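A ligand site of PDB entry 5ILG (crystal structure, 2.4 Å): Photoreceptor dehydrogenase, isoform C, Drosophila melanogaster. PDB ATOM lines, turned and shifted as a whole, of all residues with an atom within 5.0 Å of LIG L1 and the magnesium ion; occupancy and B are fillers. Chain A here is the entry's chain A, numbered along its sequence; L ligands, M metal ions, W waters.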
ATOM      1  N   GLY A  22      -6.028 -25.156   0.377  1.00  0.00           N
ATOM      2  CA  GLY A  22      -6.970 -24.341   1.158  1.00  0.00           C
ATOM      3  C   GLY A  22      -8.069 -23.723   0.299  1.00  0.00           C
ATOM      4  O   GLY A  22      -8.741 -22.787   0.724  1.00  0.00           O
ATOM      5  N   ALA A  24     -11.055 -24.650  -0.648  1.00  0.00           N
ATOM      6  CA  ALA A  24     -12.473 -24.938  -0.390  1.00  0.00           C
ATOM      7  C   ALA A  24     -13.172 -23.897   0.437  1.00  0.00           C
ATOM      8  O   ALA A  24     -14.389 -23.973   0.671  1.00  0.00           O
ATOM      9  CB  ALA A  24     -12.606 -26.278   0.294  1.00  0.00           C
ATOM     10  N   GLY A  25     -12.412 -22.940   0.933  1.00  0.00           N
ATOM     11  CA  GLY A  25     -12.972 -21.901   1.800  1.00  0.00           C
ATOM     12  C   GLY A  25     -12.149 -20.662   1.891  1.00  0.00           C
ATOM     13  O   GLY A  25     -11.027 -20.596   1.387  1.00  0.00           O
ATOM     14  N   GLY A  26     -12.753 -19.656   2.514  1.00  0.00           N
ATOM     15  CA  GLY A  26     -12.170 -18.330   2.665  1.00  0.00           C
ATOM     16  C   GLY A  26     -11.454 -17.766   1.458  1.00  0.00           C
ATOM     17  O   GLY A  26     -11.998 -17.751   0.358  1.00  0.00           O
ATOM     18  N   ILE A  27     -10.199 -17.381   1.669  1.00  0.00           N
ATOM     19  CA  ILE A  27      -9.374 -16.761   0.635  1.00  0.00           C
ATOM     20  C   ILE A  27      -9.121 -17.689  -0.530  1.00  0.00           C
ATOM     21  O   ILE A  27      -9.257 -17.284  -1.701  1.00  0.00           O
ATOM     22  CB  ILE A  27      -8.014 -16.318   1.210  1.00  0.00           C
ATOM     23  CG1 ILE A  27      -8.220 -15.170   2.214  1.00  0.00           C
ATOM     24  CG2 ILE A  27      -7.092 -15.838   0.107  1.00  0.00           C
ATOM     25  CD1 ILE A  27      -7.022 -14.850   3.074  1.00  0.00           C
ATOM     26  N   GLY A  28      -8.680 -18.898  -0.215  1.00  0.00           N
ATOM     27  CA  GLY A  28      -8.436 -19.946  -1.206  1.00  0.00           C
ATOM     28  C   GLY A  28      -9.616 -20.258  -2.117  1.00  0.00           C
ATOM     29  O   GLY A  28      -9.441 -20.526  -3.285  1.00  0.00           O
ATOM     30  N   ILE A  46      -6.877 -28.692  -3.133  1.00  0.00           N
ATOM     31  CA  ILE A  46      -6.398 -29.548  -2.067  1.00  0.00           C
ATOM     32  C   ILE A  46      -6.858 -28.931  -0.762  1.00  0.00           C
ATOM     33  O   ILE A  46      -6.447 -27.838  -0.399  1.00  0.00           O
ATOM     34  CB  ILE A  46      -4.869 -29.704  -2.081  1.00  0.00           C
ATOM     35  CG1 ILE A  46      -4.411 -30.173  -3.464  1.00  0.00           C
ATOM     36  CG2 ILE A  46      -4.435 -30.696  -1.018  1.00  0.00           C
ATOM     37  CD1 ILE A  46      -2.913 -30.332  -3.577  1.00  0.00           C
ATOM     38  N   ASP A  47      -7.720 -29.628  -0.052  1.00  0.00           N
ATOM     39  CA  ASP A  47      -8.304 -29.113   1.176  1.00  0.00           C
ATOM     40  C   ASP A  47      -8.735 -30.279   2.064  1.00  0.00           C
ATOM     41  O   ASP A  47      -8.871 -31.395   1.610  1.00  0.00           O
ATOM     42  CB  ASP A  47      -9.477 -28.178   0.842  1.00  0.00           C
ATOM     43  CG  ASP A  47      -9.811 -27.183   1.957  1.00  0.00           C
ATOM     44  OD1 ASP A  47     -10.204 -27.569   3.070  1.00  0.00           O
ATOM     45  OD2 ASP A  47      -9.706 -25.966   1.707  1.00  0.00           O
ATOM     46  N   LEU A  48      -8.922 -30.031   3.341  1.00  0.00           N
ATOM     47  CA  LEU A  48      -9.533 -31.018   4.237  1.00  0.00           C
ATOM     48  C   LEU A  48     -11.031 -31.254   3.898  1.00  0.00           C
ATOM     49  O   LEU A  48     -11.529 -32.387   4.014  1.00  0.00           O
ATOM     50  CB  LEU A  48      -9.381 -30.592   5.700  1.00  0.00           C
ATOM     51  CG  LEU A  48      -7.994 -30.716   6.318  1.00  0.00           C
ATOM     52  CD1 LEU A  48      -7.999 -30.110   7.727  1.00  0.00           C
ATOM     53  CD2 LEU A  48      -7.542 -32.166   6.341  1.00  0.00           C
ATOM     54  N   GLN A  49     -11.716 -30.180   3.496  1.00  0.00           N
ATOM     55  CA  GLN A  49     -13.159 -30.184   3.160  1.00  0.00           C
ATOM     56  C   GLN A  49     -13.397 -30.146   1.648  1.00  0.00           C
ATOM     57  O   GLN A  49     -12.593 -29.624   0.898  1.00  0.00           O
ATOM     58  CB  GLN A  49     -13.867 -28.960   3.761  1.00  0.00           C
ATOM     59  CG  GLN A  49     -13.457 -28.608   5.183  1.00  0.00           C
ATOM     60  CD  GLN A  49     -14.031 -29.532   6.245  1.00  0.00           C
ATOM     61  OE1 GLN A  49     -15.128 -30.112   6.099  1.00  0.00           O
ATOM     62  NE2 GLN A  49     -13.276 -29.656   7.347  1.00  0.00           N
ATOM     63  N   MET A  72      -7.231 -33.853   1.344  1.00  0.00           N
ATOM     64  CA  MET A  72      -5.921 -34.196   1.875  1.00  0.00           C
ATOM     65  C   MET A  72      -5.456 -33.165   2.864  1.00  0.00           C
ATOM     66  O   MET A  72      -5.659 -31.985   2.671  1.00  0.00           O
ATOM     67  CB  MET A  72      -4.903 -34.315   0.728  1.00  0.00           C
ATOM     68  CG  MET A  72      -3.483 -34.707   1.148  1.00  0.00           C
ATOM     69  SD  MET A  72      -3.430 -36.133   2.277  1.00  0.00           S
ATOM     70  CE  MET A  72      -4.162 -37.386   1.207  1.00  0.00           C
ATOM     71  N   ASP A  73      -4.834 -33.664   3.929  1.00  0.00           N
ATOM     72  CA  ASP A  73      -4.160 -32.866   4.933  1.00  0.00           C
ATOM     73  C   ASP A  73      -2.795 -32.454   4.361  1.00  0.00           C
ATOM     74  O   ASP A  73      -1.990 -33.309   4.040  1.00  0.00           O
ATOM     75  CB  ASP A  73      -3.975 -33.683   6.190  1.00  0.00           C
ATOM     76  CG  ASP A  73      -3.395 -32.893   7.342  1.00  0.00           C
ATOM     77  OD1 ASP A  73      -2.720 -31.838   7.152  1.00  0.00           O
ATOM     78  OD2 ASP A  73      -3.610 -33.352   8.482  1.00  0.00           O
ATOM     79  N   VAL A  74      -2.534 -31.160   4.252  1.00  0.00           N
ATOM     80  CA  VAL A  74      -1.242 -30.674   3.722  1.00  0.00           C
ATOM     81  C   VAL A  74      -0.023 -31.027   4.599  1.00  0.00           C
ATOM     82  O   VAL A  74       1.121 -31.025   4.121  1.00  0.00           O
ATOM     83  CB  VAL A  74      -1.227 -29.154   3.423  1.00  0.00           C
ATOM     84  CG1 VAL A  74      -2.159 -28.819   2.273  1.00  0.00           C
ATOM     85  CG2 VAL A  74      -1.563 -28.315   4.637  1.00  0.00           C
ATOM     86  N   ALA A  75      -0.272 -31.313   5.877  1.00  0.00           N
ATOM     87  CA  ALA A  75       0.793 -31.781   6.798  1.00  0.00           C
ATOM     88  C   ALA A  75       1.353 -33.157   6.415  1.00  0.00           C
ATOM     89  O   ALA A  75       2.521 -33.434   6.602  1.00  0.00           O
ATOM     90  CB  ALA A  75       0.298 -31.812   8.202  1.00  0.00           C
ATOM     91  N   VAL A 100      -2.360 -21.733   0.037  1.00  0.00           N
ATOM     92  CA  VAL A 100      -3.076 -20.842   0.950  1.00  0.00           C
ATOM     93  C   VAL A 100      -3.373 -21.538   2.270  1.00  0.00           C
ATOM     94  O   VAL A 100      -3.539 -20.879   3.286  1.00  0.00           O
ATOM     95  CB  VAL A 100      -4.417 -20.332   0.350  1.00  0.00           C
ATOM     96  CG1 VAL A 100      -5.063 -19.262   1.206  1.00  0.00           C
ATOM     97  CG2 VAL A 100      -4.163 -19.763  -1.024  1.00  0.00           C
ATOM     98  N   ALA A 101      -3.468 -22.868   2.254  1.00  0.00           N
ATOM     99  CA  ALA A 101      -3.892 -23.623   3.439  1.00  0.00           C
ATOM    100  C   ALA A 101      -3.139 -23.200   4.709  1.00  0.00           C
ATOM    101  O   ALA A 101      -1.920 -23.001   4.713  1.00  0.00           O
ATOM    102  CB  ALA A 101      -3.746 -25.102   3.216  1.00  0.00           C
ATOM    103  N   GLY A 102      -3.902 -23.015   5.762  1.00  0.00           N
ATOM    104  CA  GLY A 102      -3.369 -22.627   7.043  1.00  0.00           C
ATOM    105  C   GLY A 102      -4.458 -22.491   8.103  1.00  0.00           C
ATOM    106  O   GLY A 102      -5.619 -22.359   7.790  1.00  0.00           O
ATOM    107  N   ILE A 103      -4.037 -22.533   9.347  1.00  0.00           N
ATOM    108  CA  ILE A 103      -4.921 -22.457  10.505  1.00  0.00           C
ATOM    109  C   ILE A 103      -4.369 -21.438  11.512  1.00  0.00           C
ATOM    110  O   ILE A 103      -3.208 -21.091  11.472  1.00  0.00           O
ATOM    111  CB  ILE A 103      -5.177 -23.838  11.174  1.00  0.00           C
ATOM    112  CG1 ILE A 103      -3.885 -24.560  11.521  1.00  0.00           C
ATOM    113  CG2 ILE A 103      -5.955 -24.751  10.232  1.00  0.00           C
ATOM    114  CD1 ILE A 103      -3.619 -24.774  12.984  1.00  0.00           C
ATOM    115  N   PHE A 104      -5.257 -20.891  12.337  1.00  0.00           N
ATOM    116  CA  PHE A 104      -4.822 -20.244  13.574  1.00  0.00           C
ATOM    117  C   PHE A 104      -5.289 -21.088  14.774  1.00  0.00           C
ATOM    118  O   PHE A 104      -6.501 -21.317  14.933  1.00  0.00           O
ATOM    119  CB  PHE A 104      -5.305 -18.810  13.768  1.00  0.00           C
ATOM    120  CG  PHE A 104      -4.953 -18.271  15.130  1.00  0.00           C
ATOM    121  CD1 PHE A 104      -3.642 -17.897  15.415  1.00  0.00           C
ATOM    122  CD2 PHE A 104      -5.886 -18.230  16.133  1.00  0.00           C
ATOM    123  CE1 PHE A 104      -3.287 -17.482  16.683  1.00  0.00           C
ATOM    124  CE2 PHE A 104      -5.552 -17.784  17.407  1.00  0.00           C
ATOM    125  CZ  PHE A 104      -4.241 -17.395  17.683  1.00  0.00           C
ATOM    126  N   ARG A 111       0.494 -28.919  15.593  1.00  0.00           N
ATOM    127  CA  ARG A 111      -0.440 -28.773  14.460  1.00  0.00           C
ATOM    128  C   ARG A 111      -0.184 -27.492  13.661  1.00  0.00           C
ATOM    129  O   ARG A 111      -0.114 -27.532  12.445  1.00  0.00           O
ATOM    130  CB  ARG A 111      -1.886 -28.818  14.983  1.00  0.00           C
ATOM    131  CG  ARG A 111      -2.969 -28.999  13.941  1.00  0.00           C
ATOM    132  CD  ARG A 111      -2.854 -30.282  13.158  1.00  0.00           C
ATOM    133  NE  ARG A 111      -3.869 -30.316  12.114  1.00  0.00           N
ATOM    134  CZ  ARG A 111      -3.867 -31.144  11.060  1.00  0.00           C
ATOM    135  NH1 ARG A 111      -2.897 -32.016  10.841  1.00  0.00           N
ATOM    136  NH2 ARG A 111      -4.858 -31.073  10.185  1.00  0.00           N
ATOM    137  N   VAL A 115       1.066 -27.843   9.879  1.00  0.00           N
ATOM    138  CA  VAL A 115       0.119 -27.427   8.853  1.00  0.00           C
ATOM    139  C   VAL A 115       0.618 -26.176   8.152  1.00  0.00           C
ATOM    140  O   VAL A 115       0.883 -26.196   6.967  1.00  0.00           O
ATOM    141  CB  VAL A 115      -1.313 -27.220   9.389  1.00  0.00           C
ATOM    142  CG1 VAL A 115      -2.227 -26.564   8.348  1.00  0.00           C
ATOM    143  CG2 VAL A 115      -1.878 -28.552   9.836  1.00  0.00           C
ATOM    144  N   ASN A 116       0.759 -25.090   8.907  1.00  0.00           N
ATOM    145  CA  ASN A 116       1.091 -23.775   8.312  1.00  0.00           C
ATOM    146  C   ASN A 116       2.445 -23.730   7.637  1.00  0.00           C
ATOM    147  O   ASN A 116       2.600 -23.092   6.572  1.00  0.00           O
ATOM    148  CB  ASN A 116       1.051 -22.648   9.349  1.00  0.00           C
ATOM    149  CG  ASN A 116      -0.364 -22.353   9.819  1.00  0.00           C
ATOM    150  OD1 ASN A 116      -1.295 -23.025   9.417  1.00  0.00           O
ATOM    151  ND2 ASN A 116      -0.516 -21.347  10.657  1.00  0.00           N
ATOM    152  N   MET A 145       1.427 -18.352   0.819  1.00  0.00           N
ATOM    153  CA  MET A 145       0.679 -17.517   1.714  1.00  0.00           C
ATOM    154  C   MET A 145       1.377 -17.358   3.067  1.00  0.00           C
ATOM    155  O   MET A 145       1.327 -18.224   3.928  1.00  0.00           O
ATOM    156  CB  MET A 145      -0.705 -18.074   1.941  1.00  0.00           C
ATOM    157  CG  MET A 145      -1.543 -17.325   2.961  1.00  0.00           C
ATOM    158  SD  MET A 145      -1.928 -15.637   2.508  1.00  0.00           S
ATOM    159  CE  MET A 145      -3.078 -15.837   1.190  1.00  0.00           C
ATOM    160  N   SER A 146       1.965 -16.168   3.234  1.00  0.00           N
ATOM    161  CA  SER A 146       2.479 -15.706   4.522  1.00  0.00           C
ATOM    162  C   SER A 146       1.472 -14.721   5.092  1.00  0.00           C
ATOM    163  O   SER A 146       0.294 -14.787   4.795  1.00  0.00           O
ATOM    164  CB  SER A 146       3.893 -15.107   4.377  1.00  0.00           C
ATOM    165  OG  SER A 146       4.398 -14.733   5.670  1.00  0.00           O
ATOM    166  N   SER A 147       1.936 -13.833   5.950  1.00  0.00           N
ATOM    167  CA  SER A 147       1.119 -12.778   6.563  1.00  0.00           C
ATOM    168  C   SER A 147       2.011 -11.582   6.867  1.00  0.00           C
ATOM    169  O   SER A 147       3.228 -11.730   7.017  1.00  0.00           O
ATOM    170  CB  SER A 147       0.533 -13.313   7.869  1.00  0.00           C
ATOM    171  OG  SER A 147      -0.077 -12.318   8.663  1.00  0.00           O
ATOM    172  N   TYR A 160       1.748 -18.895  15.520  1.00  0.00           N
ATOM    173  CA  TYR A 160       1.270 -18.547  14.187  1.00  0.00           C
ATOM    174  C   TYR A 160       2.293 -17.685  13.415  1.00  0.00           C
ATOM    175  O   TYR A 160       2.640 -17.981  12.267  1.00  0.00           O
ATOM    176  CB  TYR A 160      -0.069 -17.823  14.286  1.00  0.00           C
ATOM    177  CG  TYR A 160      -0.619 -17.312  12.984  1.00  0.00           C
ATOM    178  CD1 TYR A 160      -1.344 -18.145  12.131  1.00  0.00           C
ATOM    179  CD2 TYR A 160      -0.426 -16.008  12.579  1.00  0.00           C
ATOM    180  CE1 TYR A 160      -1.873 -17.669  10.920  1.00  0.00           C
ATOM    181  CE2 TYR A 160      -0.912 -15.530  11.381  1.00  0.00           C
ATOM    182  CZ  TYR A 160      -1.656 -16.360  10.553  1.00  0.00           C
ATOM    183  OH  TYR A 160      -2.135 -15.888   9.344  1.00  0.00           O
ATOM    184  N   LYS A 164       4.547 -17.998   9.888  1.00  0.00           N
ATOM    185  CA  LYS A 164       4.451 -17.023   8.792  1.00  0.00           C
ATOM    186  C   LYS A 164       5.790 -16.454   8.375  1.00  0.00           C
ATOM    187  O   LYS A 164       6.061 -16.234   7.206  1.00  0.00           O
ATOM    188  CB  LYS A 164       3.456 -15.899   9.141  1.00  0.00           C
ATOM    189  CG  LYS A 164       2.027 -16.388   9.170  1.00  0.00           C
ATOM    190  CD  LYS A 164       1.550 -16.977   7.844  1.00  0.00           C
ATOM    191  CE  LYS A 164       0.848 -18.312   8.041  1.00  0.00           C
ATOM    192  NZ  LYS A 164       0.346 -18.907   6.761  1.00  0.00           N
ATOM    193  N   PRO A 192      -0.721 -10.767   3.535  1.00  0.00           N
ATOM    194  CA  PRO A 192      -1.887  -9.962   3.789  1.00  0.00           C
ATOM    195  C   PRO A 192      -2.072  -9.549   5.221  1.00  0.00           C
ATOM    196  O   PRO A 192      -1.678 -10.270   6.171  1.00  0.00           O
ATOM    197  CB  PRO A 192      -3.061 -10.861   3.341  1.00  0.00           C
ATOM    198  CG  PRO A 192      -2.433 -12.029   2.631  1.00  0.00           C
ATOM    199  CD  PRO A 192      -1.083 -12.167   3.239  1.00  0.00           C
ATOM    200  N   GLY A 193      -2.713  -8.396   5.386  1.00  0.00           N
ATOM    201  CA  GLY A 193      -3.199  -7.973   6.700  1.00  0.00           C
ATOM    202  C   GLY A 193      -4.518  -8.658   7.055  1.00  0.00           C
ATOM    203  O   GLY A 193      -5.041  -9.468   6.309  1.00  0.00           O
ATOM    204  N   ALA A 194      -5.033  -8.287   8.199  1.00  0.00           N
ATOM    205  CA  ALA A 194      -6.314  -8.786   8.707  1.00  0.00           C
ATOM    206  C   ALA A 194      -7.370  -8.830   7.610  1.00  0.00           C
ATOM    207  O   ALA A 194      -7.537  -7.900   6.836  1.00  0.00           O
ATOM    208  CB  ALA A 194      -6.803  -7.916   9.862  1.00  0.00           C
ATOM    209  N   THR A 195      -8.111  -9.903   7.607  1.00  0.00           N
ATOM    210  CA  THR A 195      -9.098 -10.228   6.562  1.00  0.00           C
ATOM    211  C   THR A 195     -10.193 -11.036   7.232  1.00  0.00           C
ATOM    212  O   THR A 195      -9.945 -12.028   7.875  1.00  0.00           O
ATOM    213  CB  THR A 195      -8.478 -11.055   5.414  1.00  0.00           C
ATOM    214  OG1 THR A 195      -7.305 -10.394   4.948  1.00  0.00           O
ATOM    215  CG2 THR A 195      -9.462 -11.181   4.271  1.00  0.00           C
ATOM    216  N   MET A 196     -11.425 -10.584   7.072  1.00  0.00           N
ATOM    217  CA  MET A 196     -12.580 -11.256   7.677  1.00  0.00           C
ATOM    218  C   MET A 196     -12.842 -12.683   7.073  1.00  0.00           C
ATOM    219  O   MET A 196     -13.339 -12.814   5.981  1.00  0.00           O
ATOM    220  CB  MET A 196     -13.814 -10.351   7.542  1.00  0.00           C
ATOM    221  CG  MET A 196     -15.101 -10.862   8.137  1.00  0.00           C
ATOM    222  SD  MET A 196     -14.936 -11.667   9.728  1.00  0.00           S
ATOM    223  CE  MET A 196     -16.170 -12.915   9.415  1.00  0.00           C
ATOM    224  N   THR A 197     -12.460 -13.719   7.811  1.00  0.00           N
ATOM    225  CA  THR A 197     -12.606 -15.125   7.389  1.00  0.00           C
ATOM    226  C   THR A 197     -12.875 -15.993   8.594  1.00  0.00           C
ATOM    227  O   THR A 197     -12.773 -15.540   9.714  1.00  0.00           O
ATOM    228  CB  THR A 197     -11.332 -15.689   6.688  1.00  0.00           C
ATOM    229  OG1 THR A 197     -10.280 -15.862   7.625  1.00  0.00           O
ATOM    230  CG2 THR A 197     -10.866 -14.802   5.543  1.00  0.00           C
ATOM    231  N   ASP A 198     -13.196 -17.246   8.328  1.00  0.00           N
ATOM    232  CA  ASP A 198     -13.409 -18.234   9.391  1.00  0.00           C
ATOM    233  C   ASP A 198     -12.173 -18.503  10.269  1.00  0.00           C
ATOM    234  O   ASP A 198     -12.294 -19.139  11.324  1.00  0.00           O
ATOM    235  CB  ASP A 198     -13.887 -19.574   8.815  1.00  0.00           C
ATOM    236  CG  ASP A 198     -14.319 -20.578   9.896  1.00  0.00           C
ATOM    237  OD1 ASP A 198     -15.169 -20.162  10.696  1.00  0.00           O
ATOM    238  OD2 ASP A 198     -13.797 -21.749   9.992  1.00  0.00           O
ATOM    239  N   MET A 199     -10.987 -18.060   9.838  1.00  0.00           N
ATOM    240  CA  MET A 199      -9.767 -18.213  10.671  1.00  0.00           C
ATOM    241  C   MET A 199      -9.901 -17.556  12.048  1.00  0.00           C
ATOM    242  O   MET A 199      -9.322 -18.031  13.028  1.00  0.00           O
ATOM    243  CB  MET A 199      -8.525 -17.667   9.963  1.00  0.00           C
ATOM    244  CG  MET A 199      -7.223 -18.064  10.664  1.00  0.00           C
ATOM    245  SD  MET A 199      -5.671 -17.534   9.926  1.00  0.00           S
ATOM    246  CE  MET A 199      -5.750 -15.799  10.281  1.00  0.00           C
ATOM    247  N   PHE A 200     -10.688 -16.484  12.110  1.00  0.00           N
ATOM    248  CA  PHE A 200     -10.912 -15.719  13.332  1.00  0.00           C
ATOM    249  C   PHE A 200     -12.105 -16.154  14.162  1.00  0.00           C
ATOM    250  O   PHE A 200     -12.379 -15.542  15.176  1.00  0.00           O
ATOM    251  CB  PHE A 200     -10.984 -14.220  13.016  1.00  0.00           C
ATOM    252  CG  PHE A 200      -9.681 -13.672  12.518  1.00  0.00           C
ATOM    253  CD1 PHE A 200      -8.587 -13.537  13.374  1.00  0.00           C
ATOM    254  CD2 PHE A 200      -9.507 -13.373  11.190  1.00  0.00           C
ATOM    255  CE1 PHE A 200      -7.374 -13.075  12.918  1.00  0.00           C
ATOM    256  CE2 PHE A 200      -8.302 -12.894  10.718  1.00  0.00           C
ATOM    257  CZ  PHE A 200      -7.222 -12.750  11.579  1.00  0.00           C
HETATM  258  P1  LIG L   1     -10.178 -20.277   6.284  1.00  0.00           P
HETATM  259  O1  LIG L   1      -9.864 -21.036   7.538  1.00  0.00           O
HETATM  260  O2  LIG L   1     -11.593 -20.196   5.834  1.00  0.00           O
HETATM  261  O3  LIG L   1      -9.376 -20.889   5.053  1.00  0.00           O
HETATM  262  C1  LIG L   1      -8.439 -21.948   5.243  1.00  0.00           C
HETATM  263  C2  LIG L   1      -8.747 -23.088   4.291  1.00  0.00           C
HETATM  264  O4  LIG L   1      -7.651 -24.005   4.311  1.00  0.00           O
HETATM  265  C3  LIG L   1      -9.974 -23.849   4.746  1.00  0.00           C
HETATM  266  O5  LIG L   1     -10.763 -24.193   3.609  1.00  0.00           O
HETATM  267  C4  LIG L   1      -9.420 -25.094   5.389  1.00  0.00           C
HETATM  268  O6  LIG L   1     -10.291 -26.211   5.212  1.00  0.00           O
HETATM  269  C5  LIG L   1      -8.119 -25.300   4.649  1.00  0.00           C
HETATM  270  N1  LIG L   1      -7.171 -26.021   5.518  1.00  0.00           N
HETATM  271  C6  LIG L   1      -6.861 -25.724   6.789  1.00  0.00           C
HETATM  272  N2  LIG L   1      -5.971 -26.600   7.291  1.00  0.00           N
HETATM  273  C7  LIG L   1      -5.706 -27.499   6.326  1.00  0.00           C
HETATM  274  C8  LIG L   1      -4.851 -28.696   6.187  1.00  0.00           C
HETATM  275  N3  LIG L   1      -4.083 -29.128   7.198  1.00  0.00           N
HETATM  276  N4  LIG L   1      -4.877 -29.342   5.001  1.00  0.00           N
HETATM  277  C9  LIG L   1      -5.632 -28.928   3.982  1.00  0.00           C
HETATM  278  N5  LIG L   1      -6.427 -27.854   4.038  1.00  0.00           N
HETATM  279  C10 LIG L   1      -6.503 -27.113   5.162  1.00  0.00           C
HETATM  280  O7  LIG L   1      -9.655 -18.763   6.429  1.00  0.00           O
HETATM  281  P2  LIG L   1      -8.429 -18.055   5.665  1.00  0.00           P
HETATM  282  O8  LIG L   1      -8.576 -18.245   4.202  1.00  0.00           O
HETATM  283  O9  LIG L   1      -8.337 -16.662   6.185  1.00  0.00           O
HETATM  284  O10 LIG L   1      -7.105 -18.787   6.203  1.00  0.00           O
HETATM  285  C11 LIG L   1      -6.210 -19.457   5.331  1.00  0.00           C
HETATM  286  C12 LIG L   1      -4.838 -18.800   5.265  1.00  0.00           C
HETATM  287  O11 LIG L   1      -4.947 -17.388   5.124  1.00  0.00           O
HETATM  288  C13 LIG L   1      -3.950 -19.058   6.472  1.00  0.00           C
HETATM  289  O12 LIG L   1      -2.818 -19.807   6.052  1.00  0.00           O
HETATM  290  C14 LIG L   1      -3.449 -17.693   6.895  1.00  0.00           C
HETATM  291  O13 LIG L   1      -2.055 -17.714   7.165  1.00  0.00           O
HETATM  292  C15 LIG L   1      -3.776 -16.825   5.692  1.00  0.00           C
HETATM  293  N6  LIG L   1      -3.939 -15.426   6.068  1.00  0.00           N
HETATM  294  C16 LIG L   1      -5.093 -15.006   6.567  1.00  0.00           C
HETATM  295  C17 LIG L   1      -5.243 -13.682   6.942  1.00  0.00           C
HETATM  296  C18 LIG L   1      -6.555 -13.210   7.496  1.00  0.00           C
HETATM  297  O14 LIG L   1      -6.565 -12.379   8.377  1.00  0.00           O
HETATM  298  N7  LIG L   1      -7.667 -13.747   7.017  1.00  0.00           N
HETATM  299  C19 LIG L   1      -4.201 -12.789   6.782  1.00  0.00           C
HETATM  300  C20 LIG L   1      -3.007 -13.271   6.271  1.00  0.00           C
HETATM  301  C21 LIG L   1      -2.897 -14.603   5.926  1.00  0.00           C
HETATM  302  C1  LG2 L   2      -2.846 -12.434  10.230  1.00  0.00           C
HETATM  303  C2  LG2 L   2      -3.335 -12.690  11.523  1.00  0.00           C
HETATM  304  C3  LG2 L   2      -3.720 -11.638  12.359  1.00  0.00           C
HETATM  305  C4  LG2 L   2      -3.610 -10.324  11.912  1.00  0.00           C
HETATM  306  C5  LG2 L   2      -3.100 -10.104  10.626  1.00  0.00           C
HETATM  307  C6  LG2 L   2      -2.742 -11.145   9.796  1.00  0.00           C
HETATM  308  O1  LG2 L   2      -2.481 -13.511   9.408  1.00  0.00           O
HETATM  309 MG    MG M   1      -8.049 -21.427   9.069  1.00  0.00          MG
HETATM  310  O   HOH W   1     -13.372 -18.201   5.679  1.00  0.00           O
HETATM  311  O   HOH W   2      -8.472 -20.198   2.489  1.00  0.00           O
HETATM  312  O   HOH W   3      -5.710 -28.385   9.823  1.00  0.00           O
HETATM  313  O   HOH W   4     -11.337 -27.592   7.557  1.00  0.00           O
HETATM  314  O   HOH W   5     -12.071 -22.851   8.337  1.00  0.00           O
HETATM  315  O   HOH W   6      -8.142 -21.611  12.094  1.00  0.00           O
HETATM  316  O   HOH W   7     -13.564 -22.001   5.598  1.00  0.00           O
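Residues that only touch LIG L1: Gly 22, Ala 24, Gly 26, Gln 49, Met 72, Ala 101, Ile 103, Arg 111, Val 115, Met 145, Ser 146, Ser 147, Pro 192, Gly 193, Ala 194, Asp 198, Met 199 and Phe 200.
Hydrophobic or aromatic side chains within 4 Å of LIG L1: Ile 27, Leu 48, Val 74, Ala 101, Ile 103, Val 115, Met 145, Tyr 160, Pro 192, Met 199 and Phe 200.
Of the 36 residues printed, 30 come within 4 Å of LIG L1.
The nearest printed residue that does not touch LIG L1 is Ile 46 (4.4 Å).
The backbone carbonyl oxygen (O) of Asp 47 lies within hydrogen-bond range of the backbone NH (N) of Met 72, 3.0 Å away.
The side-chain carboxylate of Asp 47 is in hydrogen-bond range of the backbone NH of Ala 24.
OG1 of Thr 197 sits close to N of Met 199, 3.2 Å away.
NZ of Lys 164 is in hydrogen-bond range of O of Met 145 (3.1 Å).
OD2 of Asp 73 lies within salt-bridge range of NH1 of Arg 111.
The side-chain carboxylate (OD1) of Asp 73 sits at hydrogen-bond distance from the backbone NH (N) of Ala 75 (2.8 Å).
N of Gly 22 is in hydrogen-bond range of O of Ile 46.
OD1 of Asn 116 sits at hydrogen-bond distance from N of Ile 103 (2.8 Å).
Water W2 lies within hydrogen-bond range of an oxygen (O8) of LIG L1, the backbone carbonyl oxygen (O) of Gly 25, the backbone NH (N) of Gly 28, the backbone carbonyl oxygen (O) of Gly 22 and the backbone NH (N) of Ile 27.
Water W1 lies within hydrogen-bond range of an oxygen (O2) of LIG L1 (2.7 Å) and the backbone NH (N) of Asp 198 (2.8 Å).
Water W4 lies within hydrogen-bond range of NE2 of Gln 49 (2.8 Å) and O6 of LIG L1 (2.9 Å).
Water W3 bridges NH2 of Arg 111 (2.8 Å) and N2 of LIG L1 (3.1 Å).
Residues that only touch the magnesium ion: Gly 102 (2.9 Å), Ile 103 (3.6 Å) and Met 199 (3.8 Å).
O6 of LIG L1 lies within hydrogen-bond range of OD1 of Asp 47 (2.5 Å).
An oxygen (O9) of LIG L1 sits at hydrogen-bond distance from the side-chain hydroxyl (OG1) of Thr 197, 2.5 Å away.
The side-chain amino group (NZ) of Lys 164 lies within hydrogen-bond range of an oxygen (O13) of LIG L1 (2.7 Å).
The side-chain hydroxyl of Tyr 160 is in hydrogen-bond range of an oxygen (O13) of LIG L1.
The backbone NH (N) of Gly 102 lies close to an oxygen (O12) of LIG L1, at 3.4 Å.
The backbone NH of Thr 195 sits at hydrogen-bond distance from an oxygen (O14) of LIG L1.
The backbone carbonyl oxygen of Thr 195 lies within hydrogen-bond range of a nitrogen (N7) of LIG L1, at 3.0 Å.
A nitrogen (N3) of LIG L1 is in hydrogen-bond range of the side-chain carboxylate (OD1) of Asp 73, at 3.0 Å.
O of Val 100 lies within hydrogen-bond range of O12 of LIG L1 (3.1 Å).
The backbone NH (N) of Val 74 is in hydrogen-bond range of a nitrogen (N4) of LIG L1, 3.1 Å away.
The backbone NH (N) of Ile 27 sits at hydrogen-bond distance from an oxygen (O8) of LIG L1 (3.1 Å).
N of Gly 25 is in hydrogen-bond range of O5 of LIG L1, 3.4 Å away.
The backbone NH of Leu 48 sits at hydrogen-bond distance from a nitrogen (N5) of LIG L1.
An oxygen (O1) of LG2 L2 sits at hydrogen-bond distance from the side-chain hydroxyl of Tyr 160, 2.4 Å away.
The side-chain hydroxyl (OG) of Ser 147 is in hydrogen-bond range of an oxygen (O1) of LG2 L2, at 2.8 Å.
The magnesium ion is bound by O1 of LIG L1.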
